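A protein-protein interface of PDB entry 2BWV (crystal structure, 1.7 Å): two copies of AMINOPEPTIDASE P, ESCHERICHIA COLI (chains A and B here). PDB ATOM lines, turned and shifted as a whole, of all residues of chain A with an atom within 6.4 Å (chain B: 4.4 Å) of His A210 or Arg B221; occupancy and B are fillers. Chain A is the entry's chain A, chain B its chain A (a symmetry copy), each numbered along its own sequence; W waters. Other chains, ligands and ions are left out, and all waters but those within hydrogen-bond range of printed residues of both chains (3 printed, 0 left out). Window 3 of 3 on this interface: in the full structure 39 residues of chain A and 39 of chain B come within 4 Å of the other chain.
The backbone carbonyl oxygen (O) of Tyr A209 is in hydrogen-bond range of the side-chain amide nitrogen (ND2) of Asn B220 (2.9 Å).
A ring nitrogen (NE2) of His A210 sits at hydrogen-bond distance from the backbone carbonyl oxygen of Arg B221 (2.9 Å).
A ring nitrogen (NE2) of His B217 is in hydrogen-bond range of the side-chain carboxylate of Glu A214 (2.8 Å).
Among the printed residues, merely in contact across the chains: Tyr A209 with Gly B223, His A210 with Asn B220, Gly A213 with His B217 and Gly A213 with Asn B220.
Of chain B, only Asn B220 and Arg B221 come within 4 Å of His A210.
Of chain A, only His A210 (2.9 Å) comes within 4 Å of Arg B221.
Of the printed residues of chain A, Gly B223 touches Tyr A209 (3.6 Å).
Of the printed residues of chain A, Asn B220 touches Tyr A209, His A210 and Gly A213.
Of the printed residues of chain A, His B217 touches Gly A213 (3.5 Å) and Glu A214 (2.8 Å).
Of the printed residues of chain B, Gly A213 touches His B217 and Asn B220.
Printed residues of chain B within 4 Å of Tyr A209: Asn B220 and Gly B223.
The nearest printed residue of chain B that does not touch His A210 is His B222 (4.9 Å).
No position is printed for both chains.
A ring nitrogen (ND1) of His A210 is in hydrogen-bond range of the backbone NH (N) of Phe A207 (3.1 Å).
The backbone NH (N) of Tyr A209 sits at hydrogen-bond distance from the backbone carbonyl oxygen (O) of Asn A247 (3.0 Å).
The side-chain carboxylate (OE1) of Glu B218 lies within salt-bridge range of the guanidinium group (NE) of Arg B221, 2.9 Å away.
Of the 13 printed residues of chain A, 4 touch a printed residue of chain B.
Hydrophobic or aromatic side chains of chain B within 4 Å of the printed part of chain A: His B217.
Among the printed residues, no Asp or Glu carboxylate lies within 4 Å of a Lys or Arg side-chain nitrogen of the other chain.
Water W1 lies within hydrogen-bond range of OH of Tyr A209 (2.7 Å), O of Arg B221 (2.8 Å) and NE2 of His A210 (3.3 Å).
Water W2 bridges the backbone carbonyl oxygen (O) of Gly A213 and the backbone NH (N) of His B217.
Water W3 lies within hydrogen-bond range of the side-chain amide nitrogen of Asn B220 and the side-chain carboxylate of Glu A212.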
ATOM      1  N   GLY A 205     -24.602 -27.687 -24.955  1.00  0.00           N
ATOM      2  CA  GLY A 205     -24.142 -29.085 -25.094  1.00  0.00           C
ATOM      3  C   GLY A 205     -22.632 -29.237 -25.186  1.00  0.00           C
ATOM      4  O   GLY A 205     -22.081 -30.308 -24.889  1.00  0.00           O
ATOM      5  N   MET A 206     -21.955 -28.188 -25.642  1.00  0.00           N
ATOM      6  CA  MET A 206     -20.503 -28.148 -25.570  1.00  0.00           C
ATOM      7  C   MET A 206     -20.086 -28.076 -24.111  1.00  0.00           C
ATOM      8  O   MET A 206     -20.810 -27.541 -23.268  1.00  0.00           O
ATOM      9  CB  MET A 206     -19.955 -26.934 -26.338  1.00  0.00           C
ATOM     10  CG  MET A 206     -20.075 -27.127 -27.854  1.00  0.00           C
ATOM     11  SD  MET A 206     -19.573 -25.665 -28.773  1.00  0.00           S
ATOM     12  CE  MET A 206     -18.019 -25.284 -27.995  1.00  0.00           C
ATOM     13  N   PHE A 207     -18.923 -28.631 -23.814  1.00  0.00           N
ATOM     14  CA  PHE A 207     -18.338 -28.518 -22.489  1.00  0.00           C
ATOM     15  C   PHE A 207     -17.569 -27.197 -22.328  1.00  0.00           C
ATOM     16  O   PHE A 207     -17.039 -26.622 -23.296  1.00  0.00           O
ATOM     17  CB  PHE A 207     -17.427 -29.709 -22.202  1.00  0.00           C
ATOM     18  CG  PHE A 207     -18.189 -30.964 -21.881  1.00  0.00           C
ATOM     19  CD1 PHE A 207     -18.742 -31.734 -22.899  1.00  0.00           C
ATOM     20  CD2 PHE A 207     -18.433 -31.309 -20.563  1.00  0.00           C
ATOM     21  CE1 PHE A 207     -19.490 -32.877 -22.596  1.00  0.00           C
ATOM     22  CE2 PHE A 207     -19.163 -32.434 -20.250  1.00  0.00           C
ATOM     23  CZ  PHE A 207     -19.703 -33.218 -21.267  1.00  0.00           C
ATOM     24  N   GLU A 208     -17.488 -26.740 -21.080  1.00  0.00           N
ATOM     25  CA  GLU A 208     -16.749 -25.529 -20.757  1.00  0.00           C
ATOM     26  C   GLU A 208     -15.330 -25.617 -21.349  1.00  0.00           C
ATOM     27  O   GLU A 208     -14.848 -24.671 -21.959  1.00  0.00           O
ATOM     28  CB  GLU A 208     -16.701 -25.334 -19.233  1.00  0.00           C
ATOM     29  CG  GLU A 208     -18.066 -24.921 -18.649  1.00  0.00           C
ATOM     30  CD  GLU A 208     -18.183 -25.102 -17.139  1.00  0.00           C
ATOM     31  OE1 GLU A 208     -17.449 -25.938 -16.548  1.00  0.00           O
ATOM     32  OE2 GLU A 208     -19.055 -24.412 -16.563  1.00  0.00           O
ATOM     33  N   TYR A 209     -14.690 -26.782 -21.185  1.00  0.00           N
ATOM     34  CA  TYR A 209     -13.319 -26.962 -21.681  1.00  0.00           C
ATOM     35  C   TYR A 209     -13.191 -26.824 -23.206  1.00  0.00           C
ATOM     36  O   TYR A 209     -12.118 -26.483 -23.702  1.00  0.00           O
ATOM     37  CB  TYR A 209     -12.688 -28.258 -21.189  1.00  0.00           C
ATOM     38  CG  TYR A 209     -13.334 -29.539 -21.639  1.00  0.00           C
ATOM     39  CD1 TYR A 209     -13.126 -30.052 -22.926  1.00  0.00           C
ATOM     40  CD2 TYR A 209     -14.127 -30.278 -20.765  1.00  0.00           C
ATOM     41  CE1 TYR A 209     -13.683 -31.251 -23.327  1.00  0.00           C
ATOM     42  CE2 TYR A 209     -14.715 -31.487 -21.171  1.00  0.00           C
ATOM     43  CZ  TYR A 209     -14.490 -31.967 -22.455  1.00  0.00           C
ATOM     44  OH  TYR A 209     -15.046 -33.157 -22.877  1.00  0.00           O
ATOM     45  N   HIS A 210     -14.278 -27.057 -23.948  1.00  0.00           N
ATOM     46  CA  HIS A 210     -14.236 -26.840 -25.402  1.00  0.00           C
ATOM     47  C   HIS A 210     -13.906 -25.382 -25.765  1.00  0.00           C
ATOM     48  O   HIS A 210     -13.160 -25.131 -26.703  1.00  0.00           O
ATOM     49  CB  HIS A 210     -15.504 -27.308 -26.102  1.00  0.00           C
ATOM     50  CG  HIS A 210     -15.624 -28.800 -26.199  1.00  0.00           C
ATOM     51  ND1 HIS A 210     -16.781 -29.472 -25.881  1.00  0.00           N
ATOM     52  CD2 HIS A 210     -14.733 -29.743 -26.581  1.00  0.00           C
ATOM     53  CE1 HIS A 210     -16.600 -30.770 -26.066  1.00  0.00           C
ATOM     54  NE2 HIS A 210     -15.361 -30.962 -26.490  1.00  0.00           N
ATOM     55  N   LEU A 211     -14.478 -24.436 -25.025  1.00  0.00           N
ATOM     56  CA  LEU A 211     -14.168 -23.033 -25.239  1.00  0.00           C
ATOM     57  C   LEU A 211     -12.714 -22.695 -24.871  1.00  0.00           C
ATOM     58  O   LEU A 211     -12.069 -21.916 -25.569  1.00  0.00           O
ATOM     59  CB  LEU A 211     -15.180 -22.148 -24.511  1.00  0.00           C
ATOM     60  CG  LEU A 211     -16.651 -22.328 -24.930  1.00  0.00           C
ATOM     61  CD1 LEU A 211     -17.522 -21.241 -24.318  1.00  0.00           C
ATOM     62  CD2 LEU A 211     -16.811 -22.362 -26.456  1.00  0.00           C
ATOM     63  N   GLU A 212     -12.205 -23.300 -23.792  1.00  0.00           N
ATOM     64  CA  GLU A 212     -10.770 -23.231 -23.475  1.00  0.00           C
ATOM     65  C   GLU A 212      -9.940 -23.681 -24.700  1.00  0.00           C
ATOM     66  O   GLU A 212      -8.962 -23.013 -25.088  1.00  0.00           O
ATOM     67  CB  GLU A 212     -10.467 -24.078 -22.230  1.00  0.00           C
ATOM     68  CG  GLU A 212      -8.997 -24.348 -21.982  1.00  0.00           C
ATOM     69  CD  GLU A 212      -8.773 -25.184 -20.736  1.00  0.00           C
ATOM     70  OE1 GLU A 212      -9.639 -25.136 -19.836  1.00  0.00           O
ATOM     71  OE2 GLU A 212      -7.757 -25.906 -20.683  1.00  0.00           O
ATOM     72  N   GLY A 213     -10.328 -24.810 -25.299  1.00  0.00           N
ATOM     73  CA  GLY A 213      -9.628 -25.339 -26.479  1.00  0.00           C
ATOM     74  C   GLY A 213      -9.604 -24.331 -27.624  1.00  0.00           C
ATOM     75  O   GLY A 213      -8.573 -24.114 -28.239  1.00  0.00           O
ATOM     76  N   GLU A 214     -10.755 -23.737 -27.933  1.00  0.00           N
ATOM     77  CA  GLU A 214     -10.842 -22.743 -29.016  1.00  0.00           C
ATOM     78  C   GLU A 214      -9.909 -21.553 -28.722  1.00  0.00           C
ATOM     79  O   GLU A 214      -9.163 -21.090 -29.581  1.00  0.00           O
ATOM     80  CB  GLU A 214     -12.293 -22.253 -29.164  1.00  0.00           C
ATOM     81  CG  GLU A 214     -13.287 -23.320 -29.615  1.00  0.00           C
ATOM     82  CD  GLU A 214     -12.964 -23.908 -30.986  1.00  0.00           C
ATOM     83  OE1 GLU A 214     -12.697 -23.133 -31.908  1.00  0.00           O
ATOM     84  OE2 GLU A 214     -13.046 -25.148 -31.145  1.00  0.00           O
ATOM     85  N   ILE A 215      -9.955 -21.075 -27.479  1.00  0.00           N
ATOM     86  CA  ILE A 215      -9.169 -19.923 -27.035  1.00  0.00           C
ATOM     87  C   ILE A 215      -7.669 -20.198 -27.149  1.00  0.00           C
ATOM     88  O   ILE A 215      -6.917 -19.407 -27.754  1.00  0.00           O
ATOM     89  CB  ILE A 215      -9.592 -19.518 -25.596  1.00  0.00           C
ATOM     90  CG1 ILE A 215     -11.001 -18.912 -25.659  1.00  0.00           C
ATOM     91  CG2 ILE A 215      -8.600 -18.507 -24.986  1.00  0.00           C
ATOM     92  CD1 ILE A 215     -11.675 -18.725 -24.340  1.00  0.00           C
ATOM     93  N   ASN A 247     -13.559 -26.237 -15.464  1.00  0.00           N
ATOM     94  CA  ASN A 247     -14.092 -26.169 -16.838  1.00  0.00           C
ATOM     95  C   ASN A 247     -14.628 -27.519 -17.323  1.00  0.00           C
ATOM     96  O   ASN A 247     -14.413 -27.912 -18.474  1.00  0.00           O
ATOM     97  CB  ASN A 247     -13.010 -25.622 -17.778  1.00  0.00           C
ATOM     98  CG  ASN A 247     -12.507 -24.224 -17.358  1.00  0.00           C
ATOM     99  OD1 ASN A 247     -13.090 -23.567 -16.478  1.00  0.00           O
ATOM    100  ND2 ASN A 247     -11.412 -23.778 -17.978  1.00  0.00           N
ATOM    101  N   MET A 251     -22.316 -27.092 -20.947  1.00  0.00           N
ATOM    102  CA  MET A 251     -22.916 -25.759 -20.938  1.00  0.00           C
ATOM    103  C   MET A 251     -24.381 -25.868 -21.350  1.00  0.00           C
ATOM    104  O   MET A 251     -24.689 -26.441 -22.387  1.00  0.00           O
ATOM    105  CB  MET A 251     -22.155 -24.815 -21.867  1.00  0.00           C
ATOM    106  CG  MET A 251     -20.702 -24.557 -21.412  1.00  0.00           C
ATOM    107  SD  MET A 251     -19.854 -23.329 -22.378  1.00  0.00           S
ATOM    108  CE  MET A 251     -19.740 -24.182 -23.954  1.00  0.00           C
ATOM    109  N   HIS B 217      -5.446 -28.747 -29.590  1.00  0.00           N
ATOM    110  CA  HIS B 217      -6.874 -28.518 -29.826  1.00  0.00           C
ATOM    111  C   HIS B 217      -7.611 -29.854 -29.994  1.00  0.00           C
ATOM    112  O   HIS B 217      -8.680 -30.094 -29.404  1.00  0.00           O
ATOM    113  CB  HIS B 217      -7.101 -27.610 -31.031  1.00  0.00           C
ATOM    114  CG  HIS B 217      -8.545 -27.295 -31.269  1.00  0.00           C
ATOM    115  ND1 HIS B 217      -9.375 -28.112 -32.007  1.00  0.00           N
ATOM    116  CD2 HIS B 217      -9.321 -26.274 -30.825  1.00  0.00           C
ATOM    117  CE1 HIS B 217     -10.591 -27.593 -32.031  1.00  0.00           C
ATOM    118  NE2 HIS B 217     -10.587 -26.478 -31.321  1.00  0.00           N
ATOM    119  N   GLU B 218      -7.015 -30.745 -30.768  1.00  0.00           N
ATOM    120  CA  GLU B 218      -7.598 -32.080 -30.941  1.00  0.00           C
ATOM    121  C   GLU B 218      -7.670 -32.887 -29.628  1.00  0.00           C
ATOM    122  O   GLU B 218      -8.695 -33.526 -29.331  1.00  0.00           O
ATOM    123  CB  GLU B 218      -6.837 -32.876 -31.994  1.00  0.00           C
ATOM    124  CG  GLU B 218      -7.574 -34.154 -32.460  1.00  0.00           C
ATOM    125  CD  GLU B 218      -8.840 -33.870 -33.291  1.00  0.00           C
ATOM    126  OE1 GLU B 218      -9.025 -32.743 -33.802  1.00  0.00           O
ATOM    127  OE2 GLU B 218      -9.671 -34.801 -33.438  1.00  0.00           O
ATOM    128  N   PHE B 219      -6.599 -32.860 -28.832  1.00  0.00           N
ATOM    129  CA  PHE B 219      -6.649 -33.481 -27.493  1.00  0.00           C
ATOM    130  C   PHE B 219      -7.863 -32.969 -26.710  1.00  0.00           C
ATOM    131  O   PHE B 219      -8.677 -33.743 -26.189  1.00  0.00           O
ATOM    132  CB  PHE B 219      -5.419 -33.152 -26.645  1.00  0.00           C
ATOM    133  CG  PHE B 219      -4.107 -33.739 -27.133  1.00  0.00           C
ATOM    134  CD1 PHE B 219      -4.023 -34.687 -28.161  1.00  0.00           C
ATOM    135  CD2 PHE B 219      -2.923 -33.338 -26.501  1.00  0.00           C
ATOM    136  CE1 PHE B 219      -2.756 -35.205 -28.551  1.00  0.00           C
ATOM    137  CE2 PHE B 219      -1.689 -33.852 -26.890  1.00  0.00           C
ATOM    138  CZ  PHE B 219      -1.606 -34.796 -27.903  1.00  0.00           C
ATOM    139  N   ASN B 220      -7.950 -31.644 -26.618  1.00  0.00           N
ATOM    140  CA  ASN B 220      -9.003 -30.973 -25.876  1.00  0.00           C
ATOM    141  C   ASN B 220     -10.387 -31.361 -26.345  1.00  0.00           C
ATOM    142  O   ASN B 220     -11.273 -31.598 -25.530  1.00  0.00           O
ATOM    143  CB  ASN B 220      -8.810 -29.447 -25.971  1.00  0.00           C
ATOM    144  CG  ASN B 220      -9.974 -28.664 -25.377  1.00  0.00           C
ATOM    145  OD1 ASN B 220     -11.046 -28.576 -25.989  1.00  0.00           O
ATOM    146  ND2 ASN B 220      -9.775 -28.105 -24.183  1.00  0.00           N
ATOM    147  N   ARG B 221     -10.590 -31.456 -27.651  1.00  0.00           N
ATOM    148  CA  ARG B 221     -11.949 -31.669 -28.094  1.00  0.00           C
ATOM    149  C   ARG B 221     -12.503 -33.043 -27.665  1.00  0.00           C
ATOM    150  O   ARG B 221     -13.717 -33.174 -27.482  1.00  0.00           O
ATOM    151  CB  ARG B 221     -12.129 -31.352 -29.550  1.00  0.00           C
ATOM    152  CG  ARG B 221     -11.590 -32.266 -30.494  1.00  0.00           C
ATOM    153  CD  ARG B 221     -11.874 -31.679 -31.901  1.00  0.00           C
ATOM    154  NE  ARG B 221     -11.817 -32.727 -32.899  1.00  0.00           N
ATOM    155  CZ  ARG B 221     -12.854 -33.440 -33.324  1.00  0.00           C
ATOM    156  NH1 ARG B 221     -14.087 -33.190 -32.902  1.00  0.00           N
ATOM    157  NH2 ARG B 221     -12.647 -34.394 -34.222  1.00  0.00           N
ATOM    158  N   HIS B 222     -11.607 -34.005 -27.437  1.00  0.00           N
ATOM    159  CA  HIS B 222     -12.000 -35.344 -26.969  1.00  0.00           C
ATOM    160  C   HIS B 222     -11.942 -35.488 -25.439  1.00  0.00           C
ATOM    161  O   HIS B 222     -12.113 -36.573 -24.914  1.00  0.00           O
ATOM    162  CB  HIS B 222     -11.149 -36.407 -27.652  1.00  0.00           C
ATOM    163  CG  HIS B 222     -11.253 -36.362 -29.135  1.00  0.00           C
ATOM    164  ND1 HIS B 222     -12.426 -36.660 -29.798  1.00  0.00           N
ATOM    165  CD2 HIS B 222     -10.371 -35.965 -30.084  1.00  0.00           C
ATOM    166  CE1 HIS B 222     -12.240 -36.502 -31.096  1.00  0.00           C
ATOM    167  NE2 HIS B 222     -11.004 -36.083 -31.297  1.00  0.00           N
ATOM    168  N   GLY B 223     -11.680 -34.389 -24.740  1.00  0.00           N
ATOM    169  CA  GLY B 223     -11.706 -34.380 -23.277  1.00  0.00           C
ATOM    170  C   GLY B 223     -10.381 -34.709 -22.613  1.00  0.00           C
ATOM    171  O   GLY B 223     -10.352 -35.005 -21.415  1.00  0.00           O
HETATM  172  O   HOH W   1     -15.409 -34.061 -25.400  1.00  0.00           O
HETATM  173  O   HOH W   2      -6.491 -25.951 -27.813  1.00  0.00           O
HETATM  174  O   HOH W   3      -7.153 -27.757 -23.051  1.00  0.00           O
